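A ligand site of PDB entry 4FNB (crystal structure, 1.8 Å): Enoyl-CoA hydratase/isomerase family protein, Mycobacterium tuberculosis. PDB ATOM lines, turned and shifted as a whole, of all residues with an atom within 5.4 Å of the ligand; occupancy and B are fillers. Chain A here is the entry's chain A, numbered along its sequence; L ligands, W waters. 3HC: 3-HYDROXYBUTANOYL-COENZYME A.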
ATOM      1  N   LYS A  23      23.029 -13.315 -23.129  1.00  0.00           N
ATOM      2  CA  LYS A  23      21.868 -12.960 -23.940  1.00  0.00           C
ATOM      3  C   LYS A  23      21.196 -11.749 -23.324  1.00  0.00           C
ATOM      4  O   LYS A  23      21.813 -10.684 -23.213  1.00  0.00           O
ATOM      5  CB  LYS A  23      20.904 -14.140 -24.042  1.00  0.00           C
ATOM      6  CG  LYS A  23      20.063 -14.171 -25.302  1.00  0.00           C
ATOM      7  CD  LYS A  23      19.122 -15.361 -25.284  1.00  0.00           C
ATOM      8  CE  LYS A  23      18.657 -15.747 -26.664  1.00  0.00           C
ATOM      9  NZ  LYS A  23      19.805 -16.176 -27.506  1.00  0.00           N
ATOM     10  N   VAL A  24      19.936 -11.902 -22.904  1.00  0.00           N
ATOM     11  CA  VAL A  24      19.221 -10.772 -22.312  1.00  0.00           C
ATOM     12  C   VAL A  24      18.968 -10.861 -20.798  1.00  0.00           C
ATOM     13  O   VAL A  24      18.051 -10.232 -20.277  1.00  0.00           O
ATOM     14  CB  VAL A  24      17.883 -10.471 -23.057  1.00  0.00           C
ATOM     15  CG1 VAL A  24      18.175 -10.203 -24.536  1.00  0.00           C
ATOM     16  CG2 VAL A  24      16.899 -11.620 -22.906  1.00  0.00           C
ATOM     17  N   ALA A  26      17.694 -13.028 -18.784  1.00  0.00           N
ATOM     18  CA  ALA A  26      16.368 -13.454 -18.401  1.00  0.00           C
ATOM     19  C   ALA A  26      16.383 -13.914 -16.944  1.00  0.00           C
ATOM     20  O   ALA A  26      17.296 -14.630 -16.515  1.00  0.00           O
ATOM     21  CB  ALA A  26      15.859 -14.571 -19.330  1.00  0.00           C
ATOM     22  N   ARG A  57      24.402  -5.508 -23.405  1.00  0.00           N
ATOM     23  CA  ARG A  57      23.206  -5.480 -24.238  1.00  0.00           C
ATOM     24  C   ARG A  57      21.976  -4.993 -23.468  1.00  0.00           C
ATOM     25  O   ARG A  57      21.186  -4.198 -23.974  1.00  0.00           O
ATOM     26  CB  ARG A  57      22.949  -6.875 -24.814  1.00  0.00           C
ATOM     27  CG  ARG A  57      21.780  -6.953 -25.752  1.00  0.00           C
ATOM     28  CD  ARG A  57      21.586  -8.359 -26.252  1.00  0.00           C
ATOM     29  NE  ARG A  57      20.565  -8.388 -27.284  1.00  0.00           N
ATOM     30  CZ  ARG A  57      20.228  -9.478 -27.968  1.00  0.00           C
ATOM     31  NH1 ARG A  57      20.839 -10.630 -27.737  1.00  0.00           N
ATOM     32  NH2 ARG A  57      19.279  -9.403 -28.889  1.00  0.00           N
ATOM     33  N   VAL A  58      21.801  -5.483 -22.242  1.00  0.00           N
ATOM     34  CA  VAL A  58      20.632  -5.117 -21.436  1.00  0.00           C
ATOM     35  C   VAL A  58      20.974  -5.025 -19.960  1.00  0.00           C
ATOM     36  O   VAL A  58      22.012  -5.507 -19.520  1.00  0.00           O
ATOM     37  CB  VAL A  58      19.507  -6.180 -21.538  1.00  0.00           C
ATOM     38  CG1 VAL A  58      19.029  -6.354 -22.980  1.00  0.00           C
ATOM     39  CG2 VAL A  58      19.986  -7.512 -20.950  1.00  0.00           C
ATOM     40  N   SER A  60      18.151  -6.151 -18.059  1.00  0.00           N
ATOM     41  CA  SER A  60      17.467  -7.440 -18.096  1.00  0.00           C
ATOM     42  C   SER A  60      16.183  -7.370 -18.895  1.00  0.00           C
ATOM     43  O   SER A  60      15.416  -6.402 -18.777  1.00  0.00           O
ATOM     44  CB  SER A  60      17.136  -7.932 -16.684  1.00  0.00           C
ATOM     45  OG  SER A  60      16.327  -9.114 -16.730  1.00  0.00           O
ATOM     46  N   GLY A  61      15.947  -8.391 -19.714  1.00  0.00           N
ATOM     47  CA  GLY A  61      14.699  -8.528 -20.445  1.00  0.00           C
ATOM     48  C   GLY A  61      13.564  -9.137 -19.628  1.00  0.00           C
ATOM     49  O   GLY A  61      12.506  -9.441 -20.172  1.00  0.00           O
ATOM     50  N   GLY A  62      13.794  -9.325 -18.326  1.00  0.00           N
ATOM     51  CA  GLY A  62      12.734  -9.758 -17.433  1.00  0.00           C
ATOM     52  C   GLY A  62      12.635 -11.269 -17.262  1.00  0.00           C
ATOM     53  O   GLY A  62      13.613 -11.985 -17.509  1.00  0.00           O
ATOM     54  N   PHE A  63      11.485 -11.759 -16.808  1.00  0.00           N
ATOM     55  CA  PHE A  63      11.297 -13.198 -16.643  1.00  0.00           C
ATOM     56  C   PHE A  63      11.556 -13.977 -17.934  1.00  0.00           C
ATOM     57  O   PHE A  63      11.338 -13.474 -19.029  1.00  0.00           O
ATOM     58  CB  PHE A  63       9.875 -13.510 -16.133  1.00  0.00           C
ATOM     59  CG  PHE A  63       9.633 -13.088 -14.704  1.00  0.00           C
ATOM     60  CD1 PHE A  63       8.670 -12.141 -14.389  1.00  0.00           C
ATOM     61  CD2 PHE A  63      10.396 -13.634 -13.679  1.00  0.00           C
ATOM     62  CE1 PHE A  63       8.454 -11.762 -13.078  1.00  0.00           C
ATOM     63  CE2 PHE A  63      10.186 -13.263 -12.370  1.00  0.00           C
ATOM     64  CZ  PHE A  63       9.205 -12.317 -12.054  1.00  0.00           C
ATOM     65  N   ASP A  64      11.998 -15.237 -17.779  1.00  0.00           N
ATOM     66  CA  ASP A  64      12.324 -16.123 -18.897  1.00  0.00           C
ATOM     67  C   ASP A  64      11.061 -16.483 -19.660  1.00  0.00           C
ATOM     68  O   ASP A  64      10.189 -17.184 -19.146  1.00  0.00           O
ATOM     69  CB  ASP A  64      12.963 -17.403 -18.360  1.00  0.00           C
ATOM     70  CG  ASP A  64      13.497 -18.283 -19.464  1.00  0.00           C
ATOM     71  OD1 ASP A  64      13.234 -18.007 -20.649  1.00  0.00           O
ATOM     72  OD2 ASP A  64      14.177 -19.279 -19.144  1.00  0.00           O
ATOM     73  N   LEU A  65      10.964 -15.986 -20.885  1.00  0.00           N
ATOM     74  CA  LEU A  65       9.776 -16.180 -21.714  1.00  0.00           C
ATOM     75  C   LEU A  65       9.474 -17.659 -21.966  1.00  0.00           C
ATOM     76  O   LEU A  65       8.309 -18.046 -22.056  1.00  0.00           O
ATOM     77  CB  LEU A  65       9.937 -15.449 -23.041  1.00  0.00           C
ATOM     78  CG  LEU A  65       8.772 -14.643 -23.616  1.00  0.00           C
ATOM     79  CD1 LEU A  65       8.005 -13.888 -22.532  1.00  0.00           C
ATOM     80  CD2 LEU A  65       9.306 -13.683 -24.676  1.00  0.00           C
ATOM     81  N   LYS A  66      10.524 -18.459 -22.094  1.00  0.00           N
ATOM     82  CA  LYS A  66      10.372 -19.896 -22.370  1.00  0.00           C
ATOM     83  C   LYS A  66       9.574 -20.583 -21.264  1.00  0.00           C
ATOM     84  O   LYS A  66       8.653 -21.344 -21.540  1.00  0.00           O
ATOM     85  CB  LYS A  66      11.735 -20.569 -22.514  1.00  0.00           C
ATOM     86  CG  LYS A  66      12.411 -20.364 -23.866  1.00  0.00           C
ATOM     87  CD  LYS A  66      13.930 -20.344 -23.726  1.00  0.00           C
ATOM     88  CE  LYS A  66      14.392 -19.025 -23.109  1.00  0.00           C
ATOM     89  NZ  LYS A  66      15.603 -19.147 -22.243  1.00  0.00           N
ATOM     90  N   LEU A  68       7.586 -19.098 -19.155  1.00  0.00           N
ATOM     91  CA  LEU A  68       6.259 -18.499 -19.112  1.00  0.00           C
ATOM     92  C   LEU A  68       5.298 -19.076 -20.150  1.00  0.00           C
ATOM     93  O   LEU A  68       4.107 -19.222 -19.878  1.00  0.00           O
ATOM     94  CB  LEU A  68       6.334 -16.979 -19.297  1.00  0.00           C
ATOM     95  CG  LEU A  68       6.762 -16.172 -18.083  1.00  0.00           C
ATOM     96  CD1 LEU A  68       7.048 -14.733 -18.469  1.00  0.00           C
ATOM     97  CD2 LEU A  68       5.683 -16.237 -16.998  1.00  0.00           C
ATOM     98  N   LEU A  80       7.824 -16.533 -11.068  1.00  0.00           N
ATOM     99  CA  LEU A  80       7.293 -15.210 -10.717  1.00  0.00           C
ATOM    100  C   LEU A  80       7.489 -14.902  -9.232  1.00  0.00           C
ATOM    101  O   LEU A  80       7.995 -13.848  -8.872  1.00  0.00           O
ATOM    102  CB  LEU A  80       5.810 -15.086 -11.098  1.00  0.00           C
ATOM    103  CG  LEU A  80       5.502 -14.326 -12.392  1.00  0.00           C
ATOM    104  CD1 LEU A  80       6.329 -14.823 -13.560  1.00  0.00           C
ATOM    105  CD2 LEU A  80       4.015 -14.391 -12.708  1.00  0.00           C
ATOM    106  N   PHE A  84       9.791 -11.842  -7.562  1.00  0.00           N
ATOM    107  CA  PHE A  84       9.286 -10.786  -6.694  1.00  0.00           C
ATOM    108  C   PHE A  84       9.866 -10.908  -5.287  1.00  0.00           C
ATOM    109  O   PHE A  84      10.045  -9.902  -4.604  1.00  0.00           O
ATOM    110  CB  PHE A  84       7.753 -10.731  -6.698  1.00  0.00           C
ATOM    111  CG  PHE A  84       7.179 -10.285  -8.020  1.00  0.00           C
ATOM    112  CD1 PHE A  84       7.553  -9.065  -8.559  1.00  0.00           C
ATOM    113  CD2 PHE A  84       6.294 -11.084  -8.719  1.00  0.00           C
ATOM    114  CE1 PHE A  84       7.037  -8.636  -9.783  1.00  0.00           C
ATOM    115  CE2 PHE A  84       5.779 -10.668  -9.937  1.00  0.00           C
ATOM    116  CZ  PHE A  84       6.148  -9.452 -10.470  1.00  0.00           C
ATOM    117  N   HIS A 104      18.702  -1.908 -21.823  1.00  0.00           N
ATOM    118  CA  HIS A 104      17.251  -1.868 -21.601  1.00  0.00           C
ATOM    119  C   HIS A 104      16.821  -2.691 -20.376  1.00  0.00           C
ATOM    120  O   HIS A 104      17.455  -3.677 -20.012  1.00  0.00           O
ATOM    121  CB  HIS A 104      16.494  -2.342 -22.840  1.00  0.00           C
ATOM    122  CG  HIS A 104      17.000  -1.732 -24.118  1.00  0.00           C
ATOM    123  ND1 HIS A 104      17.000  -0.379 -24.342  1.00  0.00           N
ATOM    124  CD2 HIS A 104      17.552  -2.296 -25.222  1.00  0.00           C
ATOM    125  CE1 HIS A 104      17.518  -0.124 -25.532  1.00  0.00           C
ATOM    126  NE2 HIS A 104      17.859  -1.279 -26.083  1.00  0.00           N
ATOM    127  N   ILE A 106      13.225  -4.320 -19.140  1.00  0.00           N
ATOM    128  CA  ILE A 106      11.846  -4.537 -19.602  1.00  0.00           C
ATOM    129  C   ILE A 106      11.098  -5.472 -18.645  1.00  0.00           C
ATOM    130  O   ILE A 106      11.624  -6.518 -18.253  1.00  0.00           O
ATOM    131  CB  ILE A 106      11.811  -5.146 -21.030  1.00  0.00           C
ATOM    132  CG1 ILE A 106      12.680  -4.343 -22.016  1.00  0.00           C
ATOM    133  CG2 ILE A 106      10.355  -5.280 -21.525  1.00  0.00           C
ATOM    134  CD1 ILE A 106      12.220  -2.887 -22.235  1.00  0.00           C
ATOM    135  N   ALA A 107       9.866  -5.103 -18.287  1.00  0.00           N
ATOM    136  CA  ALA A 107       9.039  -5.946 -17.448  1.00  0.00           C
ATOM    137  C   ALA A 107       9.741  -6.256 -16.126  1.00  0.00           C
ATOM    138  O   ALA A 107      10.101  -5.330 -15.410  1.00  0.00           O
ATOM    139  CB  ALA A 107       8.650  -7.230 -18.204  1.00  0.00           C
ATOM    140  N   MET A 108       9.957  -7.522 -15.771  1.00  0.00           N
ATOM    141  CA  MET A 108      10.607  -7.793 -14.480  1.00  0.00           C
ATOM    142  C   MET A 108      12.000  -7.154 -14.397  1.00  0.00           C
ATOM    143  O   MET A 108      12.509  -6.876 -13.321  1.00  0.00           O
ATOM    144  CB  MET A 108      10.675  -9.283 -14.150  1.00  0.00           C
ATOM    145  CG  MET A 108      11.192  -9.580 -12.747  1.00  0.00           C
ATOM    146  SD  MET A 108      10.092  -9.046 -11.403  1.00  0.00           S
ATOM    147  CE  MET A 108      11.302  -8.648 -10.124  1.00  0.00           C
ATOM    148  N   PHE A 111      11.155  -3.945 -13.079  1.00  0.00           N
ATOM    149  CA  PHE A 111      10.724  -4.055 -11.689  1.00  0.00           C
ATOM    150  C   PHE A 111      11.943  -4.250 -10.796  1.00  0.00           C
ATOM    151  O   PHE A 111      12.054  -3.643  -9.732  1.00  0.00           O
ATOM    152  CB  PHE A 111       9.700  -5.187 -11.515  1.00  0.00           C
ATOM    153  CG  PHE A 111       8.566  -5.109 -12.485  1.00  0.00           C
ATOM    154  CD1 PHE A 111       8.119  -3.880 -12.942  1.00  0.00           C
ATOM    155  CD2 PHE A 111       7.976  -6.261 -12.976  1.00  0.00           C
ATOM    156  CE1 PHE A 111       7.090  -3.803 -13.870  1.00  0.00           C
ATOM    157  CE2 PHE A 111       6.935  -6.192 -13.904  1.00  0.00           C
ATOM    158  CZ  PHE A 111       6.489  -4.965 -14.348  1.00  0.00           C
ATOM    159  N   ASN A 130       6.070  -3.677 -20.314  1.00  0.00           N
ATOM    160  CA  ASN A 130       5.380  -3.907 -21.584  1.00  0.00           C
ATOM    161  C   ASN A 130       4.224  -4.907 -21.451  1.00  0.00           C
ATOM    162  O   ASN A 130       3.615  -5.309 -22.448  1.00  0.00           O
ATOM    163  CB  ASN A 130       6.368  -4.382 -22.643  1.00  0.00           C
ATOM    164  CG  ASN A 130       6.850  -5.813 -22.386  1.00  0.00           C
ATOM    165  OD1 ASN A 130       6.858  -6.266 -21.249  1.00  0.00           O
ATOM    166  ND2 ASN A 130       7.216  -6.511 -23.448  1.00  0.00           N
ATOM    167  N   GLU A 131       3.924  -5.291 -20.220  1.00  0.00           N
ATOM    168  CA  GLU A 131       2.931  -6.332 -19.965  1.00  0.00           C
ATOM    169  C   GLU A 131       1.612  -6.083 -20.687  1.00  0.00           C
ATOM    170  O   GLU A 131       1.083  -6.977 -21.370  1.00  0.00           O
ATOM    171  CB  GLU A 131       2.669  -6.492 -18.452  1.00  0.00           C
ATOM    172  CG  GLU A 131       3.663  -7.361 -17.692  1.00  0.00           C
ATOM    173  CD  GLU A 131       4.973  -6.661 -17.375  1.00  0.00           C
ATOM    174  OE1 GLU A 131       5.182  -5.505 -17.800  1.00  0.00           O
ATOM    175  OE2 GLU A 131       5.820  -7.291 -16.708  1.00  0.00           O
ATOM    176  N   ILE A 134       1.648  -6.685 -24.441  1.00  0.00           N
ATOM    177  CA  ILE A 134       1.759  -8.046 -24.951  1.00  0.00           C
ATOM    178  C   ILE A 134       0.659  -8.998 -24.429  1.00  0.00           C
ATOM    179  O   ILE A 134       0.671 -10.193 -24.728  1.00  0.00           O
ATOM    180  CB  ILE A 134       3.182  -8.615 -24.720  1.00  0.00           C
ATOM    181  CG1 ILE A 134       3.534  -8.644 -23.223  1.00  0.00           C
ATOM    182  CG2 ILE A 134       4.205  -7.760 -25.459  1.00  0.00           C
ATOM    183  CD1 ILE A 134       3.161  -9.922 -22.512  1.00  0.00           C
ATOM    184  N   MET A 136      -0.616  -9.175 -20.916  1.00  0.00           N
ATOM    185  CA  MET A 136      -0.591  -9.595 -19.526  1.00  0.00           C
ATOM    186  C   MET A 136      -1.041  -8.463 -18.614  1.00  0.00           C
ATOM    187  O   MET A 136      -0.618  -7.313 -18.770  1.00  0.00           O
ATOM    188  CB  MET A 136       0.799 -10.057 -19.119  1.00  0.00           C
ATOM    189  CG  MET A 136       0.856 -10.422 -17.659  1.00  0.00           C
ATOM    190  SD  MET A 136       1.514 -12.069 -17.434  1.00  0.00           S
ATOM    191  CE  MET A 136       1.134 -12.343 -15.699  1.00  0.00           C
ATOM    192  N   PRO A 139       0.962  -7.936 -12.412  1.00  0.00           N
ATOM    193  CA  PRO A 139       0.742  -8.474 -11.063  1.00  0.00           C
ATOM    194  C   PRO A 139       0.795  -7.367  -9.999  1.00  0.00           C
ATOM    195  O   PRO A 139       1.506  -6.363 -10.158  1.00  0.00           O
ATOM    196  CB  PRO A 139       1.930  -9.432 -10.876  1.00  0.00           C
ATOM    197  CG  PRO A 139       2.360  -9.801 -12.285  1.00  0.00           C
ATOM    198  CD  PRO A 139       2.133  -8.532 -13.073  1.00  0.00           C
HETATM  199  N1A 3HC L   1      13.156 -14.507 -22.033  1.00  0.00           N
HETATM  200  C2A 3HC L   1      13.711 -15.350 -22.877  1.00  0.00           C
HETATM  201  N3A 3HC L   1      14.192 -15.001 -24.042  1.00  0.00           N
HETATM  202  C4A 3HC L   1      14.120 -13.753 -24.484  1.00  0.00           C
HETATM  203  C5A 3HC L   1      13.518 -12.734 -23.606  1.00  0.00           C
HETATM  204  C6A 3HC L   1      13.007 -13.198 -22.312  1.00  0.00           C
HETATM  205  N6A 3HC L   1      12.424 -12.381 -21.421  1.00  0.00           N
HETATM  206  N7A 3HC L   1      13.629 -11.575 -24.265  1.00  0.00           N
HETATM  207  C8A 3HC L   1      14.206 -11.832 -25.449  1.00  0.00           C
HETATM  208  N9A 3HC L   1      14.505 -13.132 -25.568  1.00  0.00           N
HETATM  209  C1B 3HC L   1      15.208 -13.737 -26.727  1.00  0.00           C
HETATM  210  C2B 3HC L   1      14.523 -13.600 -28.076  1.00  0.00           C
HETATM  211  O2B 3HC L   1      13.528 -14.552 -28.180  1.00  0.00           O
HETATM  212  C3B 3HC L   1      15.724 -13.726 -29.004  1.00  0.00           C
HETATM  213  O3B 3HC L   1      16.264 -14.987 -28.842  1.00  0.00           O
HETATM  214  P3B 3HC L   1      17.177 -15.615 -29.961  1.00  0.00           P
HETATM  215  O7A 3HC L   1      17.705 -16.874 -29.351  1.00  0.00           O
HETATM  216  O8A 3HC L   1      18.336 -14.709 -30.240  1.00  0.00           O
HETATM  217  O9A 3HC L   1      16.079 -15.738 -31.025  1.00  0.00           O
HETATM  218  C4B 3HC L   1      16.753 -12.912 -28.246  1.00  0.00           C
HETATM  219  O4B 3HC L   1      16.458 -13.104 -26.894  1.00  0.00           O
HETATM  220  C5B 3HC L   1      16.679 -11.429 -28.449  1.00  0.00           C
HETATM  221  O5B 3HC L   1      15.368 -11.088 -28.805  1.00  0.00           O
HETATM  222  P1A 3HC L   1      15.063  -9.754 -29.579  1.00  0.00           P
HETATM  223  O1A 3HC L   1      13.783  -9.179 -29.119  1.00  0.00           O
HETATM  224  O2A 3HC L   1      15.243 -10.059 -31.001  1.00  0.00           O
HETATM  225  O3A 3HC L   1      16.250  -8.835 -29.123  1.00  0.00           O
HETATM  226  P2A 3HC L   1      16.288  -7.251 -29.122  1.00  0.00           P
HETATM  227  O4A 3HC L   1      15.451  -6.741 -30.222  1.00  0.00           O
HETATM  228  O5A 3HC L   1      17.710  -6.955 -28.836  1.00  0.00           O
HETATM  229  O6A 3HC L   1      15.539  -6.855 -27.766  1.00  0.00           O
HETATM  230  CBP 3HC L   1      14.727  -6.997 -25.552  1.00  0.00           C
HETATM  231  CCP 3HC L   1      15.822  -7.402 -26.512  1.00  0.00           C
HETATM  232  CDP 3HC L   1      14.641  -5.497 -25.432  1.00  0.00           C
HETATM  233  CEP 3HC L   1      15.037  -7.466 -24.140  1.00  0.00           C
HETATM  234  CAP 3HC L   1      13.438  -7.633 -26.062  1.00  0.00           C
HETATM  235  OAP 3HC L   1      13.697  -8.943 -26.466  1.00  0.00           O
HETATM  236  C9P 3HC L   1      12.304  -7.605 -25.059  1.00  0.00           C
HETATM  237  O9P 3HC L   1      11.761  -6.589 -24.864  1.00  0.00           O
HETATM  238  N8P 3HC L   1      11.947  -8.674 -24.403  1.00  0.00           N
HETATM  239  C7P 3HC L   1      10.932  -8.592 -23.395  1.00  0.00           C
HETATM  240  C6P 3HC L   1      10.144  -9.866 -23.280  1.00  0.00           C
HETATM  241  C5P 3HC L   1       8.758  -9.719 -22.783  1.00  0.00           C
HETATM  242  O5P 3HC L   1       7.882  -9.418 -23.529  1.00  0.00           O
HETATM  243  N4P 3HC L   1       8.616 -10.000 -21.505  1.00  0.00           N
HETATM  244  C3P 3HC L   1       7.455  -9.687 -20.733  1.00  0.00           C
HETATM  245  C2P 3HC L   1       6.507 -10.849 -20.776  1.00  0.00           C
HETATM  246  S1P 3HC L   1       5.249 -10.777 -19.541  1.00  0.00           S
HETATM  247  C1  3HC L   1       5.959 -11.447 -18.231  1.00  0.00           C
HETATM  248  O1  3HC L   1       7.037 -11.906 -18.392  1.00  0.00           O
HETATM  249  C2  3HC L   1       5.259 -11.481 -16.873  1.00  0.00           C
HETATM  250  C3  3HC L   1       5.784 -10.634 -15.697  1.00  0.00           C
HETATM  251  O3  3HC L   1       6.655  -9.594 -16.088  1.00  0.00           O
HETATM  252  C4  3HC L   1       4.655 -10.092 -14.829  1.00  0.00           C
HETATM  253  O   HOH W   1       9.186 -10.092 -17.019  1.00  0.00           O
HETATM  254  O   HOH W   2      13.734  -4.530 -29.640  1.00  0.00           O
HETATM  255  O   HOH W   3      19.533 -18.076 -31.363  1.00  0.00           O
HETATM  256  O   HOH W   4      14.344 -14.469 -32.599  1.00  0.00           O
HETATM  257  O   HOH W   5      10.373 -10.926 -19.572  1.00  0.00           O
HETATM  258  O   HOH W   6      11.179  -4.257 -26.144  1.00  0.00           O
HETATM  259  O   HOH W   7      13.568 -15.988 -30.271  1.00  0.00           O
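Water W1 lies within hydrogen-bond range of O3 of the ligand (2.7 Å), N of Phe 63 (2.8 Å) and N of Met 108 (3.0 Å).
Water W5 lies within hydrogen-bond range of O of Gly 61 (2.7 Å), N4P of the ligand (2.8 Å) and O of Phe 63 (2.8 Å).
Merely in contact with the ligand: Val 24, Ala 26, Asp 64, Lys 66, Leu 68, Ile 106, Ala 107, Met 108, Ile 134, Met 136 and Pro 139.
Within 4 Å of the ligand: Lys 23, Val 24, Ala 26, Arg 57, Gly 61, Phe 63, Asp 64, Leu 65, Lys 66, Leu 68, Ile 106, Ala 107, Met 108, Asn 130, Glu 131, Ile 134, Met 136 and Pro 139.
A nitrogen (N1A) of the ligand lies within hydrogen-bond range of the backbone NH of Leu 65 (2.9 Å).
O5A of the ligand is in salt-bridge range of NH2 of Arg 57 (2.9 Å).
N6A of the ligand lies within hydrogen-bond range of O of Phe 63 (2.8 Å).
NZ of Lys 23 lies within salt-bridge range of O7A of the ligand (2.9 Å).
The side-chain carboxylate (OE2) of Glu 131 is in hydrogen-bond range of an oxygen (O3) of the ligand, at 2.5 Å.
The side-chain amide nitrogen of Asn 130 is in hydrogen-bond range of an oxygen (O5P) of the ligand, 3.0 Å away.
O of Gly 61 lies within hydrogen-bond range of N6A of the ligand.
N of Ile 106 is in hydrogen-bond range of O of Ser 60 (3.0 Å).
The backbone NH of Met 136 sits at hydrogen-bond distance from the backbone carbonyl oxygen of Glu 131 (2.8 Å).
The backbone carbonyl oxygen (O) of Val 24 sits at hydrogen-bond distance from the backbone NH (N) of Gly 61 (2.9 Å).
The side-chain carboxylate (OD1) of Asp 64 lies within salt-bridge range of the side-chain amino group (NZ) of Lys 66.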
